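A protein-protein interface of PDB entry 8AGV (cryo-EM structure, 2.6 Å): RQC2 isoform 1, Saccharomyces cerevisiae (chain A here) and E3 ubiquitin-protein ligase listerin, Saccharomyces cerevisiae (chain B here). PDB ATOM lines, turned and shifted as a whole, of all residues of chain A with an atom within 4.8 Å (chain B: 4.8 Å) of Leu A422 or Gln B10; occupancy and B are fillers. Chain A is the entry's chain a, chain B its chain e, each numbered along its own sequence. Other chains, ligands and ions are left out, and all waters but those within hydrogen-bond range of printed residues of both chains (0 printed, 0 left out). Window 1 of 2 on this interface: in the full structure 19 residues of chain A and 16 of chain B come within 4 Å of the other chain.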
ATOM      1  N   LEU A 409       2.414  -3.013   5.131  1.00  0.00           N
ATOM      2  CA  LEU A 409       3.641  -2.488   5.714  1.00  0.00           C
ATOM      3  C   LEU A 409       4.408  -1.635   4.717  1.00  0.00           C
ATOM      4  O   LEU A 409       4.942  -0.588   5.073  1.00  0.00           O
ATOM      5  CB  LEU A 409       4.528  -3.617   6.229  1.00  0.00           C
ATOM      6  CG  LEU A 409       4.275  -4.152   7.638  1.00  0.00           C
ATOM      7  CD1 LEU A 409       4.103  -2.992   8.601  1.00  0.00           C
ATOM      8  CD2 LEU A 409       3.064  -5.065   7.691  1.00  0.00           C
ATOM      9  N   THR A 418      13.238  -3.028   9.178  1.00  0.00           N
ATOM     10  CA  THR A 418      12.322  -3.033  10.307  1.00  0.00           C
ATOM     11  C   THR A 418      11.180  -3.989  10.042  1.00  0.00           C
ATOM     12  O   THR A 418      10.725  -4.682  10.946  1.00  0.00           O
ATOM     13  CB  THR A 418      11.765  -1.639  10.630  1.00  0.00           C
ATOM     14  OG1 THR A 418      10.772  -1.274   9.665  1.00  0.00           O
ATOM     15  CG2 THR A 418      12.880  -0.606  10.636  1.00  0.00           C
ATOM     16  N   ILE A 419      10.714  -4.031   8.802  1.00  0.00           N
ATOM     17  CA  ILE A 419       9.603  -4.900   8.472  1.00  0.00           C
ATOM     18  C   ILE A 419      10.008  -6.338   8.739  1.00  0.00           C
ATOM     19  O   ILE A 419       9.256  -7.095   9.345  1.00  0.00           O
ATOM     20  CB  ILE A 419       9.190  -4.747   6.995  1.00  0.00           C
ATOM     21  CG1 ILE A 419       8.624  -3.352   6.738  1.00  0.00           C
ATOM     22  CG2 ILE A 419       8.157  -5.792   6.600  1.00  0.00           C
ATOM     23  CD1 ILE A 419       8.301  -3.087   5.284  1.00  0.00           C
ATOM     24  N   GLU A 420      11.220  -6.704   8.340  1.00  0.00           N
ATOM     25  CA  GLU A 420      11.686  -8.069   8.554  1.00  0.00           C
ATOM     26  C   GLU A 420      11.797  -8.421  10.028  1.00  0.00           C
ATOM     27  O   GLU A 420      11.451  -9.527  10.429  1.00  0.00           O
ATOM     28  CB  GLU A 420      13.005  -8.332   7.831  1.00  0.00           C
ATOM     29  CG  GLU A 420      12.855  -8.421   6.322  1.00  0.00           C
ATOM     30  CD  GLU A 420      14.029  -9.110   5.658  1.00  0.00           C
ATOM     31  OE1 GLU A 420      14.919  -9.596   6.385  1.00  0.00           O
ATOM     32  OE2 GLU A 420      14.057  -9.172   4.412  1.00  0.00           O
ATOM     33  N   LYS A 421      12.263  -7.483  10.840  1.00  0.00           N
ATOM     34  CA  LYS A 421      12.361  -7.732  12.268  1.00  0.00           C
ATOM     35  C   LYS A 421      10.969  -8.003  12.791  1.00  0.00           C
ATOM     36  O   LYS A 421      10.778  -8.860  13.652  1.00  0.00           O
ATOM     37  CB  LYS A 421      12.973  -6.537  12.990  1.00  0.00           C
ATOM     38  CG  LYS A 421      14.463  -6.368  12.759  1.00  0.00           C
ATOM     39  CD  LYS A 421      15.239  -7.545  13.325  1.00  0.00           C
ATOM     40  CE  LYS A 421      14.989  -7.707  14.817  1.00  0.00           C
ATOM     41  NZ  LYS A 421      15.504  -6.557  15.611  1.00  0.00           N
ATOM     42  N   LEU A 422       9.993  -7.274  12.275  1.00  0.00           N
ATOM     43  CA  LEU A 422       8.616  -7.496  12.681  1.00  0.00           C
ATOM     44  C   LEU A 422       8.160  -8.902  12.314  1.00  0.00           C
ATOM     45  O   LEU A 422       7.491  -9.561  13.101  1.00  0.00           O
ATOM     46  CB  LEU A 422       7.701  -6.463  12.032  1.00  0.00           C
ATOM     47  CG  LEU A 422       6.207  -6.564  12.325  1.00  0.00           C
ATOM     48  CD1 LEU A 422       5.980  -6.646  13.823  1.00  0.00           C
ATOM     49  CD2 LEU A 422       5.480  -5.373  11.724  1.00  0.00           C
ATOM     50  N   ILE A 423       8.532  -9.379  11.134  1.00  0.00           N
ATOM     51  CA  ILE A 423       8.061 -10.689  10.721  1.00  0.00           C
ATOM     52  C   ILE A 423       8.592 -11.688  11.729  1.00  0.00           C
ATOM     53  O   ILE A 423       7.874 -12.586  12.168  1.00  0.00           O
ATOM     54  CB  ILE A 423       8.574 -11.083   9.322  1.00  0.00           C
ATOM     55  CG1 ILE A 423       8.281  -9.989   8.298  1.00  0.00           C
ATOM     56  CG2 ILE A 423       7.955 -12.397   8.870  1.00  0.00           C
ATOM     57  CD1 ILE A 423       6.811  -9.712   8.097  1.00  0.00           C
ATOM     58  N   LYS A 424       9.844 -11.513  12.130  1.00  0.00           N
ATOM     59  CA  LYS A 424      10.446 -12.448  13.066  1.00  0.00           C
ATOM     60  C   LYS A 424       9.703 -12.423  14.380  1.00  0.00           C
ATOM     61  O   LYS A 424       9.425 -13.470  14.960  1.00  0.00           O
ATOM     62  CB  LYS A 424      11.907 -12.087  13.309  1.00  0.00           C
ATOM     63  CG  LYS A 424      12.752 -12.040  12.052  1.00  0.00           C
ATOM     64  CD  LYS A 424      14.134 -11.478  12.329  1.00  0.00           C
ATOM     65  CE  LYS A 424      14.905 -11.280  11.034  1.00  0.00           C
ATOM     66  NZ  LYS A 424      16.262 -10.716  11.274  1.00  0.00           N
ATOM     67  N   SER A 425       9.355 -11.232  14.845  1.00  0.00           N
ATOM     68  CA  SER A 425       8.685 -11.115  16.127  1.00  0.00           C
ATOM     69  C   SER A 425       7.356 -11.824  16.070  1.00  0.00           C
ATOM     70  O   SER A 425       6.988 -12.534  16.997  1.00  0.00           O
ATOM     71  CB  SER A 425       8.472  -9.651  16.479  1.00  0.00           C
ATOM     72  OG  SER A 425       8.018  -9.509  17.810  1.00  0.00           O
ATOM     73  N   GLU A 426       6.646 -11.662  14.964  1.00  0.00           N
ATOM     74  CA  GLU A 426       5.356 -12.314  14.802  1.00  0.00           C
ATOM     75  C   GLU A 426       5.480 -13.827  14.810  1.00  0.00           C
ATOM     76  O   GLU A 426       4.611 -14.516  15.327  1.00  0.00           O
ATOM     77  CB  GLU A 426       4.655 -11.833  13.533  1.00  0.00           C
ATOM     78  CG  GLU A 426       4.255 -10.367  13.572  1.00  0.00           C
ATOM     79  CD  GLU A 426       3.270 -10.056  14.682  1.00  0.00           C
ATOM     80  OE1 GLU A 426       2.400 -10.905  14.962  1.00  0.00           O
ATOM     81  OE2 GLU A 426       3.357  -8.957  15.268  1.00  0.00           O
ATOM     82  N   ASN B   7      -2.047  -1.937   9.439  1.00  0.00           N
ATOM     83  CA  ASN B   7      -1.273  -2.901  10.217  1.00  0.00           C
ATOM     84  C   ASN B   7      -2.013  -4.223  10.270  1.00  0.00           C
ATOM     85  O   ASN B   7      -2.552  -4.595  11.309  1.00  0.00           O
ATOM     86  CB  ASN B   7      -1.036  -2.383  11.635  1.00  0.00           C
ATOM     87  CG  ASN B   7       0.122  -1.412  11.716  1.00  0.00           C
ATOM     88  OD1 ASN B   7       1.151  -1.602  11.069  1.00  0.00           O
ATOM     89  ND2 ASN B   7      -0.031  -0.374  12.530  1.00  0.00           N
ATOM     90  N   THR B   8      -2.032  -4.941   9.155  1.00  0.00           N
ATOM     91  CA  THR B   8      -2.745  -6.210   9.089  1.00  0.00           C
ATOM     92  C   THR B   8      -2.166  -7.251  10.031  1.00  0.00           C
ATOM     93  O   THR B   8      -2.909  -7.992  10.672  1.00  0.00           O
ATOM     94  CB  THR B   8      -2.724  -6.765   7.658  1.00  0.00           C
ATOM     95  OG1 THR B   8      -2.483  -5.696   6.735  1.00  0.00           O
ATOM     96  CG2 THR B   8      -4.048  -7.431   7.325  1.00  0.00           C
ATOM     97  N   PHE B   9      -0.843  -7.296  10.139  1.00  0.00           N
ATOM     98  CA  PHE B   9      -0.198  -8.299  10.979  1.00  0.00           C
ATOM     99  C   PHE B   9      -0.628  -8.160  12.428  1.00  0.00           C
ATOM    100  O   PHE B   9      -0.846  -9.157  13.111  1.00  0.00           O
ATOM    101  CB  PHE B   9       1.321  -8.171  10.894  1.00  0.00           C
ATOM    102  CG  PHE B   9       1.948  -9.040   9.846  1.00  0.00           C
ATOM    103  CD1 PHE B   9       2.151 -10.387  10.082  1.00  0.00           C
ATOM    104  CD2 PHE B   9       2.346  -8.509   8.634  1.00  0.00           C
ATOM    105  CE1 PHE B   9       2.733 -11.192   9.125  1.00  0.00           C
ATOM    106  CE2 PHE B   9       2.931  -9.308   7.671  1.00  0.00           C
ATOM    107  CZ  PHE B   9       3.123 -10.652   7.916  1.00  0.00           C
ATOM    108  N   GLN B  10      -0.749  -6.926  12.902  1.00  0.00           N
ATOM    109  CA  GLN B  10      -1.169  -6.692  14.279  1.00  0.00           C
ATOM    110  C   GLN B  10      -2.576  -7.215  14.530  1.00  0.00           C
ATOM    111  O   GLN B  10      -2.867  -7.732  15.608  1.00  0.00           O
ATOM    112  CB  GLN B  10      -1.061  -5.209  14.634  1.00  0.00           C
ATOM    113  CG  GLN B  10       0.314  -4.616  14.370  1.00  0.00           C
ATOM    114  CD  GLN B  10       1.425  -5.327  15.122  1.00  0.00           C
ATOM    115  OE1 GLN B  10       1.250  -5.749  16.265  1.00  0.00           O
ATOM    116  NE2 GLN B  10       2.581  -5.451  14.483  1.00  0.00           N
ATOM    117  N   GLN B  11      -3.453  -7.069  13.544  1.00  0.00           N
ATOM    118  CA  GLN B  11      -4.817  -7.560  13.686  1.00  0.00           C
ATOM    119  C   GLN B  11      -4.814  -9.062  13.884  1.00  0.00           C
ATOM    120  O   GLN B  11      -5.580  -9.579  14.690  1.00  0.00           O
ATOM    121  CB  GLN B  11      -5.632  -7.215  12.446  1.00  0.00           C
ATOM    122  CG  GLN B  11      -5.666  -5.732  12.132  1.00  0.00           C
ATOM    123  CD  GLN B  11      -6.230  -5.449  10.757  1.00  0.00           C
ATOM    124  OE1 GLN B  11      -6.454  -6.364   9.965  1.00  0.00           O
ATOM    125  NE2 GLN B  11      -6.461  -4.177  10.464  1.00  0.00           N
ATOM    126  N   TYR B  12      -3.970  -9.773  13.145  1.00  0.00           N
ATOM    127  CA  TYR B  12      -3.857 -11.214  13.348  1.00  0.00           C
ATOM    128  C   TYR B  12      -3.323 -11.525  14.735  1.00  0.00           C
ATOM    129  O   TYR B  12      -3.786 -12.461  15.384  1.00  0.00           O
ATOM    130  CB  TYR B  12      -2.928 -11.844  12.312  1.00  0.00           C
ATOM    131  CG  TYR B  12      -3.329 -11.624  10.876  1.00  0.00           C
ATOM    132  CD1 TYR B  12      -4.554 -12.067  10.399  1.00  0.00           C
ATOM    133  CD2 TYR B  12      -2.468 -10.999   9.987  1.00  0.00           C
ATOM    134  CE1 TYR B  12      -4.919 -11.873   9.082  1.00  0.00           C
ATOM    135  CE2 TYR B  12      -2.826 -10.795   8.669  1.00  0.00           C
ATOM    136  CZ  TYR B  12      -4.051 -11.238   8.220  1.00  0.00           C
ATOM    137  OH  TYR B  12      -4.408 -11.044   6.906  1.00  0.00           O
ATOM    138  N   ASN B  13      -2.350 -10.747  15.195  1.00  0.00           N
ATOM    139  CA  ASN B  13      -1.717 -11.014  16.487  1.00  0.00           C
ATOM    140  C   ASN B  13      -2.672 -10.921  17.668  1.00  0.00           C
ATOM    141  O   ASN B  13      -2.582 -11.737  18.586  1.00  0.00           O
ATOM    142  CB  ASN B  13      -0.557 -10.034  16.694  1.00  0.00           C
ATOM    143  CG  ASN B  13       0.420 -10.492  17.761  1.00  0.00           C
ATOM    144  OD1 ASN B  13       0.512 -11.680  18.071  1.00  0.00           O
ATOM    145  ND2 ASN B  13       1.169  -9.548  18.316  1.00  0.00           N
ATOM    146  N   THR B  14      -3.553  -9.924  17.670  1.00  0.00           N
ATOM    147  CA  THR B  14      -4.507  -9.722  18.775  1.00  0.00           C
ATOM    148  C   THR B  14      -3.827  -9.600  20.133  1.00  0.00           C
ATOM    149  O   THR B  14      -4.354 -10.076  21.137  1.00  0.00           O
ATOM    150  CB  THR B  14      -5.643 -10.779  18.842  1.00  0.00           C
ATOM    151  OG1 THR B  14      -5.123 -12.054  19.243  1.00  0.00           O
ATOM    152  CG2 THR B  14      -6.348 -10.912  17.505  1.00  0.00           C
ATOM    153  N   ASP B  15      -2.664  -8.961  20.175  1.00  0.00           N
ATOM    154  CA  ASP B  15      -1.995  -8.740  21.450  1.00  0.00           C
ATOM    155  C   ASP B  15      -1.850  -7.245  21.625  1.00  0.00           C
ATOM    156  O   ASP B  15      -1.298  -6.566  20.762  1.00  0.00           O
ATOM    157  CB  ASP B  15      -0.624  -9.412  21.465  1.00  0.00           C
ATOM    158  CG  ASP B  15       0.054  -9.327  22.819  1.00  0.00           C
ATOM    159  OD1 ASP B  15      -0.645  -9.111  23.831  1.00  0.00           O
ATOM    160  OD2 ASP B  15       1.291  -9.485  22.871  1.00  0.00           O
ATOM    161  N   ARG B  24      -1.896  -1.645  20.496  1.00  0.00           N
ATOM    162  CA  ARG B  24      -0.717  -2.304  21.017  1.00  0.00           C
ATOM    163  C   ARG B  24       0.306  -1.265  21.412  1.00  0.00           C
ATOM    164  O   ARG B  24       0.609  -0.362  20.637  1.00  0.00           O
ATOM    165  CB  ARG B  24      -0.120  -3.263  19.991  1.00  0.00           C
ATOM    166  CG  ARG B  24       1.213  -3.841  20.431  1.00  0.00           C
ATOM    167  CD  ARG B  24       1.697  -4.949  19.518  1.00  0.00           C
ATOM    168  NE  ARG B  24       3.014  -5.422  19.930  1.00  0.00           N
ATOM    169  CZ  ARG B  24       3.219  -6.376  20.833  1.00  0.00           C
ATOM    170  NH1 ARG B  24       2.190  -6.970  21.420  1.00  0.00           N
ATOM    171  NH2 ARG B  24       4.456  -6.736  21.146  1.00  0.00           N
ATOM    172  N   PHE B  30       9.986  -2.128  15.999  1.00  0.00           N
ATOM    173  CA  PHE B  30       9.209  -2.737  14.914  1.00  0.00           C
ATOM    174  C   PHE B  30       7.692  -2.743  15.081  1.00  0.00           C
ATOM    175  O   PHE B  30       6.968  -2.562  14.105  1.00  0.00           O
ATOM    176  CB  PHE B  30       9.737  -4.122  14.505  1.00  0.00           C
ATOM    177  CG  PHE B  30      10.382  -4.893  15.615  1.00  0.00           C
ATOM    178  CD1 PHE B  30      11.725  -4.727  15.902  1.00  0.00           C
ATOM    179  CD2 PHE B  30       9.657  -5.815  16.338  1.00  0.00           C
ATOM    180  CE1 PHE B  30      12.323  -5.444  16.914  1.00  0.00           C
ATOM    181  CE2 PHE B  30      10.248  -6.538  17.350  1.00  0.00           C
ATOM    182  CZ  PHE B  30      11.582  -6.354  17.638  1.00  0.00           C
ATOM    183  N   ASP B  31       7.201  -2.957  16.293  1.00  0.00           N
ATOM    184  CA  ASP B  31       5.754  -3.050  16.479  1.00  0.00           C
ATOM    185  C   ASP B  31       5.205  -2.091  17.516  1.00  0.00           C
ATOM    186  O   ASP B  31       5.952  -1.563  18.335  1.00  0.00           O
ATOM    187  CB  ASP B  31       5.305  -4.491  16.757  1.00  0.00           C
ATOM    188  CG  ASP B  31       6.002  -5.112  17.947  1.00  0.00           C
ATOM    189  OD1 ASP B  31       5.669  -4.753  19.092  1.00  0.00           O
ATOM    190  OD2 ASP B  31       6.861  -5.991  17.742  1.00  0.00           O
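The guanidinium group (NE) of Arg B24 lies within salt-bridge range of the side-chain carboxylate (OD1) of Asp B31, at 2.9 Å.
Among the printed residues, pairs that only touch across the chains: Leu A409 with Phe B9, Thr A418 with Phe B30, Lys A421 with Phe B30, Leu A422 with Gln B10, Leu A422 with Phe B30, Leu A422 with Asp B31, Ile A423 with Phe B9, Ser A425 with Phe B30, Ser A425 with Asp B31, Glu A426 with Gln B10 and Glu A426 with Asn B13.
Of chain B, only Gln B10, Phe B30 and Asp B31 come within 4 Å of Leu A422.
Gln B10 touches two residues of chain A.
Printed residues of chain B within 4 Å of Leu A409: Phe B9.
Printed residues of chain A within 4 Å of Phe B30: Thr A418 (3.7 Å), Lys A421 (3.6 Å), Leu A422 (3.9 Å) and Ser A425 (3.7 Å).
Of the printed residues of chain A, Phe B9 touches Leu A409 and Ile A423.
Of the printed residues of chain B, Thr A418 touches Phe B30 (3.7 Å).
Ile A419 touches none of the printed residues of chain B.
The nearest printed residue of chain B that does not touch Leu A422 is Phe B9 (5.1 Å).
The nearest printed residue of chain A that does not touch Gln B10 is Leu A409 (6.6 Å).
The nearest printed residue of chain B that does not touch Ser A425 is Arg B24 (5.6 Å).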
